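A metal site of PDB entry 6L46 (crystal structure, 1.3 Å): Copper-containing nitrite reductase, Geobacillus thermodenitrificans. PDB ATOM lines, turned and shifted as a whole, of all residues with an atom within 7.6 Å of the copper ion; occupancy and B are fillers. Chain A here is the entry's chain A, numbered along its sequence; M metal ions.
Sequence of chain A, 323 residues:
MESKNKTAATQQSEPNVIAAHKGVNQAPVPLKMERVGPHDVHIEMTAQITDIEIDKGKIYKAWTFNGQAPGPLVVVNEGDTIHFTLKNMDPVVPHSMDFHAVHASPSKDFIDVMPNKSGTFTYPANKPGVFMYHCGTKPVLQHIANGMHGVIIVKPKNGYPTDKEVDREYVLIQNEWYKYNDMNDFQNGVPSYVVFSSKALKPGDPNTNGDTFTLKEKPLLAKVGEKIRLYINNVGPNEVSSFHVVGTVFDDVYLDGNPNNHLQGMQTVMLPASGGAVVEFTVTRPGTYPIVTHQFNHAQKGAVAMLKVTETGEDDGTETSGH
The copper ion is bound by a ring nitrogen (ND1) of His 143 (1.9 Å), a ring nitrogen (ND1) of His 95 (2.0 Å), the side-chain sulfur (SG) of Cys 135 (2.2 Å) and the side-chain sulfur (SD) of Met 148 (2.6 Å).
ND2 of Asn 88 lies close to N of His 95, 3.5 Å away.
The backbone NH (N) of Met 148 lies close to the backbone carbonyl oxygen (O) of Trp 63, at 3.2 Å.
The side-chain sulfur (SG) of Cys 135 lies close to the side-chain hydroxyl (OG1) of Thr 137.
A ring nitrogen (NE2) of His 95 lies close to the backbone carbonyl oxygen (O) of Val 93, at 3.4 Å.
The side-chain carboxylate (OD2) of Asp 90 is in hydrogen-bond range of a ring nitrogen (NE2) of His 95 (2.7 Å).
The side-chain sulfur (SG) of Cys 135 sits close to the backbone NH (N) of Ser 96 (3.5 Å).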
ATOM      1  N   ALA A  47      19.054  12.492  21.818  1.00  0.00           N
ATOM      2  CA  ALA A  47      18.567  13.738  22.371  1.00  0.00           C
ATOM      3  C   ALA A  47      19.416  14.813  21.710  1.00  0.00           C
ATOM      4  O   ALA A  47      20.643  14.715  21.697  1.00  0.00           O
ATOM      5  CB  ALA A  47      18.780  13.808  23.889  1.00  0.00           C
ATOM      6  N   TRP A  63      14.447  21.214  22.451  1.00  0.00           N
ATOM      7  CA  TRP A  63      15.075  20.027  22.988  1.00  0.00           C
ATOM      8  C   TRP A  63      14.279  18.859  22.453  1.00  0.00           C
ATOM      9  O   TRP A  63      13.060  18.812  22.630  1.00  0.00           O
ATOM     10  CB  TRP A  63      14.991  20.024  24.511  1.00  0.00           C
ATOM     11  CG  TRP A  63      15.654  21.164  25.188  1.00  0.00           C
ATOM     12  CD1 TRP A  63      16.202  22.296  24.640  1.00  0.00           C
ATOM     13  CD2 TRP A  63      15.850  21.267  26.591  1.00  0.00           C
ATOM     14  NE1 TRP A  63      16.721  23.082  25.637  1.00  0.00           N
ATOM     15  CE2 TRP A  63      16.509  22.476  26.841  1.00  0.00           C
ATOM     16  CE3 TRP A  63      15.499  20.442  27.658  1.00  0.00           C
ATOM     17  CZ2 TRP A  63      16.838  22.886  28.142  1.00  0.00           C
ATOM     18  CZ3 TRP A  63      15.810  20.861  28.950  1.00  0.00           C
ATOM     19  CH2 TRP A  63      16.475  22.059  29.178  1.00  0.00           C
ATOM     20  N   THR A  64      14.960  17.944  21.767  1.00  0.00           N
ATOM     21  CA  THR A  64      14.226  16.967  20.988  1.00  0.00           C
ATOM     22  C   THR A  64      14.809  15.589  21.132  1.00  0.00           C
ATOM     23  O   THR A  64      15.975  15.400  21.505  1.00  0.00           O
ATOM     24  CB  THR A  64      14.238  17.271  19.487  1.00  0.00           C
ATOM     25  OG1 THR A  64      15.533  16.986  18.942  1.00  0.00           O
ATOM     26  CG2 THR A  64      13.883  18.716  19.191  1.00  0.00           C
ATOM     27  N   PHE A  65      13.991  14.617  20.756  1.00  0.00           N
ATOM     28  CA  PHE A  65      14.487  13.340  20.325  1.00  0.00           C
ATOM     29  C   PHE A  65      14.624  13.375  18.806  1.00  0.00           C
ATOM     30  O   PHE A  65      13.646  13.660  18.104  1.00  0.00           O
ATOM     31  CB  PHE A  65      13.534  12.233  20.737  1.00  0.00           C
ATOM     32  CG  PHE A  65      13.414  12.085  22.223  1.00  0.00           C
ATOM     33  CD1 PHE A  65      14.443  11.501  22.957  1.00  0.00           C
ATOM     34  CD2 PHE A  65      12.282  12.549  22.885  1.00  0.00           C
ATOM     35  CE1 PHE A  65      14.325  11.378  24.338  1.00  0.00           C
ATOM     36  CE2 PHE A  65      12.158  12.395  24.269  1.00  0.00           C
ATOM     37  CZ  PHE A  65      13.186  11.803  24.989  1.00  0.00           C
ATOM     38  N   LEU A  86      19.647   5.706  24.146  1.00  0.00           N
ATOM     39  CA  LEU A  86      19.604   7.148  23.958  1.00  0.00           C
ATOM     40  C   LEU A  86      21.027   7.639  23.829  1.00  0.00           C
ATOM     41  O   LEU A  86      21.847   7.428  24.718  1.00  0.00           O
ATOM     42  CB  LEU A  86      18.949   7.834  25.144  1.00  0.00           C
ATOM     43  CG  LEU A  86      18.791   9.342  24.984  1.00  0.00           C
ATOM     44  CD1 LEU A  86      17.856   9.690  23.834  1.00  0.00           C
ATOM     45  CD2 LEU A  86      18.251   9.919  26.290  1.00  0.00           C
ATOM     46  N   ASN A  88      22.933  10.977  23.766  1.00  0.00           N
ATOM     47  CA  ASN A  88      22.690  12.365  24.124  1.00  0.00           C
ATOM     48  C   ASN A  88      23.682  13.248  23.388  1.00  0.00           C
ATOM     49  O   ASN A  88      24.864  13.277  23.714  1.00  0.00           O
ATOM     50  CB  ASN A  88      22.792  12.570  25.633  1.00  0.00           C
ATOM     51  CG  ASN A  88      22.382  13.945  26.034  1.00  0.00           C
ATOM     52  OD1 ASN A  88      21.968  14.744  25.191  1.00  0.00           O
ATOM     53  ND2 ASN A  88      22.478  14.259  27.312  1.00  0.00           N
ATOM     54  N   ASP A  90      23.142  16.566  23.231  1.00  0.00           N
ATOM     55  CA  ASP A  90      23.112  17.875  23.834  1.00  0.00           C
ATOM     56  C   ASP A  90      24.468  18.117  24.475  1.00  0.00           C
ATOM     57  O   ASP A  90      24.961  17.266  25.205  1.00  0.00           O
ATOM     58  CB  ASP A  90      22.022  17.852  24.903  1.00  0.00           C
ATOM     59  CG  ASP A  90      21.740  19.210  25.518  1.00  0.00           C
ATOM     60  OD1 ASP A  90      22.700  19.962  25.795  1.00  0.00           O
ATOM     61  OD2 ASP A  90      20.556  19.499  25.772  1.00  0.00           O
ATOM     62  N   VAL A  93      23.145  19.471  28.659  1.00  0.00           N
ATOM     63  CA  VAL A  93      22.009  19.052  29.480  1.00  0.00           C
ATOM     64  C   VAL A  93      21.869  17.536  29.403  1.00  0.00           C
ATOM     65  O   VAL A  93      21.820  16.993  28.305  1.00  0.00           O
ATOM     66  CB  VAL A  93      20.690  19.727  29.055  1.00  0.00           C
ATOM     67  CG1 VAL A  93      19.614  19.399  30.077  1.00  0.00           C
ATOM     68  CG2 VAL A  93      20.858  21.226  28.927  1.00  0.00           C
ATOM     69  N   PRO A  94      21.772  16.848  30.535  1.00  0.00           N
ATOM     70  CA  PRO A  94      21.421  15.428  30.487  1.00  0.00           C
ATOM     71  C   PRO A  94      20.009  15.246  29.985  1.00  0.00           C
ATOM     72  O   PRO A  94      19.162  16.128  30.132  1.00  0.00           O
ATOM     73  CB  PRO A  94      21.507  15.000  31.960  1.00  0.00           C
ATOM     74  CG  PRO A  94      22.377  16.034  32.607  1.00  0.00           C
ATOM     75  CD  PRO A  94      21.986  17.320  31.900  1.00  0.00           C
ATOM     76  N   HIS A  95      19.747  14.064  29.428  1.00  0.00           N
ATOM     77  CA  HIS A  95      18.415  13.718  29.008  1.00  0.00           C
ATOM     78  C   HIS A  95      18.171  12.253  29.291  1.00  0.00           C
ATOM     79  O   HIS A  95      19.089  11.498  29.608  1.00  0.00           O
ATOM     80  CB  HIS A  95      18.190  14.020  27.525  1.00  0.00           C
ATOM     81  CG  HIS A  95      18.320  15.461  27.208  1.00  0.00           C
ATOM     82  ND1 HIS A  95      17.366  16.402  27.578  1.00  0.00           N
ATOM     83  CD2 HIS A  95      19.307  16.135  26.580  1.00  0.00           C
ATOM     84  CE1 HIS A  95      17.793  17.595  27.200  1.00  0.00           C
ATOM     85  NE2 HIS A  95      18.961  17.460  26.586  1.00  0.00           N
ATOM     86  N   SER A  96      16.910  11.858  29.173  1.00  0.00           N
ATOM     87  CA  SER A  96      16.515  10.514  29.518  1.00  0.00           C
ATOM     88  C   SER A  96      15.281  10.178  28.705  1.00  0.00           C
ATOM     89  O   SER A  96      14.757  11.030  27.984  1.00  0.00           O
ATOM     90  CB  SER A  96      16.183  10.413  31.000  1.00  0.00           C
ATOM     91  OG  SER A  96      15.155  11.326  31.320  1.00  0.00           O
ATOM     92  N   MET A  97      14.807   8.948  28.857  1.00  0.00           N
ATOM     93  CA  MET A  97      13.624   8.511  28.146  1.00  0.00           C
ATOM     94  C   MET A  97      12.711   7.752  29.097  1.00  0.00           C
ATOM     95  O   MET A  97      13.144   6.824  29.783  1.00  0.00           O
ATOM     96  CB  MET A  97      13.996   7.593  26.978  1.00  0.00           C
ATOM     97  CG  MET A  97      12.793   6.930  26.315  1.00  0.00           C
ATOM     98  SD  MET A  97      11.660   8.126  25.573  1.00  0.00           S
ATOM     99  CE  MET A  97      12.476   8.344  23.991  1.00  0.00           C
ATOM    100  N   ASP A 112      19.221   9.419  33.655  1.00  0.00           N
ATOM    101  CA  ASP A 112      19.855  10.382  32.787  1.00  0.00           C
ATOM    102  C   ASP A 112      21.050   9.792  32.055  1.00  0.00           C
ATOM    103  O   ASP A 112      21.795   8.973  32.577  1.00  0.00           O
ATOM    104  CB  ASP A 112      20.287  11.602  33.589  1.00  0.00           C
ATOM    105  CG  ASP A 112      19.112  12.399  34.100  1.00  0.00           C
ATOM    106  OD1 ASP A 112      18.000  12.262  33.542  1.00  0.00           O
ATOM    107  OD2 ASP A 112      19.281  13.173  35.060  1.00  0.00           O
ATOM    108  N   HIS A 134       8.508  10.516  26.751  1.00  0.00           N
ATOM    109  CA  HIS A 134       9.045  11.846  26.968  1.00  0.00           C
ATOM    110  C   HIS A 134      10.340  11.737  27.734  1.00  0.00           C
ATOM    111  O   HIS A 134      10.619  10.726  28.375  1.00  0.00           O
ATOM    112  CB  HIS A 134       8.035  12.719  27.705  1.00  0.00           C
ATOM    113  CG  HIS A 134       7.614  12.193  29.045  1.00  0.00           C
ATOM    114  ND1 HIS A 134       8.337  12.404  30.190  1.00  0.00           N
ATOM    115  CD2 HIS A 134       6.518  11.477  29.423  1.00  0.00           C
ATOM    116  CE1 HIS A 134       7.713  11.851  31.222  1.00  0.00           C
ATOM    117  NE2 HIS A 134       6.599  11.285  30.781  1.00  0.00           N
ATOM    118  N   CYS A 135      11.108  12.806  27.698  1.00  0.00           N
ATOM    119  CA  CYS A 135      12.266  12.894  28.562  1.00  0.00           C
ATOM    120  C   CYS A 135      11.811  12.947  30.013  1.00  0.00           C
ATOM    121  O   CYS A 135      10.824  13.602  30.338  1.00  0.00           O
ATOM    122  CB  CYS A 135      13.053  14.132  28.189  1.00  0.00           C
ATOM    123  SG  CYS A 135      14.506  14.351  29.188  1.00  0.00           S
ATOM    124  N   GLY A 136      12.548  12.271  30.881  1.00  0.00           N
ATOM    125  CA  GLY A 136      12.222  12.157  32.277  1.00  0.00           C
ATOM    126  C   GLY A 136      13.219  12.818  33.194  1.00  0.00           C
ATOM    127  O   GLY A 136      13.282  12.494  34.369  1.00  0.00           O
ATOM    128  N   THR A 137      13.998  13.762  32.679  1.00  0.00           N
ATOM    129  CA  THR A 137      15.041  14.425  33.438  1.00  0.00           C
ATOM    130  C   THR A 137      14.456  15.611  34.172  1.00  0.00           C
ATOM    131  O   THR A 137      13.669  16.376  33.617  1.00  0.00           O
ATOM    132  CB  THR A 137      16.122  14.866  32.459  1.00  0.00           C
ATOM    133  OG1 THR A 137      16.637  13.709  31.810  1.00  0.00           O
ATOM    134  CG2 THR A 137      17.248  15.633  33.167  1.00  0.00           C
ATOM    135  N   LYS A 138      14.825  15.760  35.427  1.00  0.00           N
ATOM    136  CA  LYS A 138      14.282  16.857  36.197  1.00  0.00           C
ATOM    137  C   LYS A 138      14.913  18.180  35.761  1.00  0.00           C
ATOM    138  O   LYS A 138      16.120  18.223  35.488  1.00  0.00           O
ATOM    139  CB  LYS A 138      14.550  16.655  37.693  1.00  0.00           C
ATOM    140  CG  LYS A 138      13.758  15.511  38.287  1.00  0.00           C
ATOM    141  CD  LYS A 138      14.017  15.357  39.770  1.00  0.00           C
ATOM    142  CE  LYS A 138      13.347  16.447  40.598  1.00  0.00           C
ATOM    143  NZ  LYS A 138      13.696  16.381  42.045  1.00  0.00           N
ATOM    144  N   PRO A 139      14.138  19.260  35.674  1.00  0.00           N
ATOM    145  CA  PRO A 139      12.691  19.305  35.877  1.00  0.00           C
ATOM    146  C   PRO A 139      11.987  18.737  34.648  1.00  0.00           C
ATOM    147  O   PRO A 139      12.211  19.197  33.515  1.00  0.00           O
ATOM    148  CB  PRO A 139      12.385  20.807  35.980  1.00  0.00           C
ATOM    149  CG  PRO A 139      13.708  21.477  36.132  1.00  0.00           C
ATOM    150  CD  PRO A 139      14.690  20.590  35.433  1.00  0.00           C
ATOM    151  N   VAL A 140      11.129  17.747  34.853  1.00  0.00           N
ATOM    152  CA  VAL A 140      10.501  17.080  33.723  1.00  0.00           C
ATOM    153  C   VAL A 140       9.682  18.066  32.912  1.00  0.00           C
ATOM    154  O   VAL A 140       9.671  18.015  31.687  1.00  0.00           O
ATOM    155  CB  VAL A 140       9.669  15.887  34.221  1.00  0.00           C
ATOM    156  CG1 VAL A 140       8.898  15.273  33.057  1.00  0.00           C
ATOM    157  CG2 VAL A 140      10.618  14.871  34.844  1.00  0.00           C
ATOM    158  N   GLN A 142      10.340  21.048  32.241  1.00  0.00           N
ATOM    159  CA  GLN A 142      11.216  21.772  31.340  1.00  0.00           C
ATOM    160  C   GLN A 142      11.573  20.932  30.125  1.00  0.00           C
ATOM    161  O   GLN A 142      11.603  21.429  28.998  1.00  0.00           O
ATOM    162  CB  GLN A 142      12.488  22.176  32.092  1.00  0.00           C
ATOM    163  CG  GLN A 142      13.402  23.057  31.293  1.00  0.00           C
ATOM    164  CD  GLN A 142      14.558  23.547  32.096  1.00  0.00           C
ATOM    165  OE1 GLN A 142      14.868  23.003  33.154  1.00  0.00           O
ATOM    166  NE2 GLN A 142      15.189  24.591  31.620  1.00  0.00           N
ATOM    167  N   HIS A 143      11.906  19.668  30.357  1.00  0.00           N
ATOM    168  CA  HIS A 143      12.300  18.819  29.255  1.00  0.00           C
ATOM    169  C   HIS A 143      11.133  18.548  28.321  1.00  0.00           C
ATOM    170  O   HIS A 143      11.300  18.564  27.093  1.00  0.00           O
ATOM    171  CB  HIS A 143      12.923  17.547  29.786  1.00  0.00           C
ATOM    172  CG  HIS A 143      14.270  17.781  30.352  1.00  0.00           C
ATOM    173  ND1 HIS A 143      15.429  17.381  29.699  1.00  0.00           N
ATOM    174  CD2 HIS A 143      14.673  18.413  31.479  1.00  0.00           C
ATOM    175  CE1 HIS A 143      16.477  17.742  30.418  1.00  0.00           C
ATOM    176  NE2 HIS A 143      16.043  18.369  31.507  1.00  0.00           N
ATOM    177  N   ILE A 144       9.942  18.308  28.871  1.00  0.00           N
ATOM    178  CA  ILE A 144       8.790  18.109  28.008  1.00  0.00           C
ATOM    179  C   ILE A 144       8.456  19.386  27.259  1.00  0.00           C
ATOM    180  O   ILE A 144       8.279  19.383  26.038  1.00  0.00           O
ATOM    181  CB  ILE A 144       7.578  17.615  28.811  1.00  0.00           C
ATOM    182  CG1 ILE A 144       7.873  16.248  29.447  1.00  0.00           C
ATOM    183  CG2 ILE A 144       6.369  17.527  27.867  1.00  0.00           C
ATOM    184  CD1 ILE A 144       6.714  15.735  30.308  1.00  0.00           C
ATOM    185  N   ASN A 146      10.114  21.896  26.407  1.00  0.00           N
ATOM    186  CA  ASN A 146      11.072  22.266  25.367  1.00  0.00           C
ATOM    187  C   ASN A 146      11.043  21.345  24.162  1.00  0.00           C
ATOM    188  O   ASN A 146      11.721  21.662  23.173  1.00  0.00           O
ATOM    189  CB  ASN A 146      12.482  22.354  25.920  1.00  0.00           C
ATOM    190  CG  ASN A 146      12.730  23.649  26.661  1.00  0.00           C
ATOM    191  OD1 ASN A 146      12.200  24.706  26.297  1.00  0.00           O
ATOM    192  ND2 ASN A 146      13.541  23.565  27.687  1.00  0.00           N
ATOM    193  N   MET A 148      10.630  17.487  24.329  1.00  0.00           N
ATOM    194  CA  MET A 148      11.033  16.079  24.441  1.00  0.00           C
ATOM    195  C   MET A 148       9.831  15.224  24.807  1.00  0.00           C
ATOM    196  O   MET A 148       9.690  14.739  25.937  1.00  0.00           O
ATOM    197  CB  MET A 148      12.165  15.919  25.436  1.00  0.00           C
ATOM    198  CG  MET A 148      13.303  16.851  25.108  1.00  0.00           C
ATOM    199  SD  MET A 148      14.859  16.455  25.884  1.00  0.00           S
ATOM    200  CE  MET A 148      15.337  14.983  25.014  1.00  0.00           C
HETATM  201 CU    CU M   1      15.584  16.025  28.316  1.00  0.00          CU
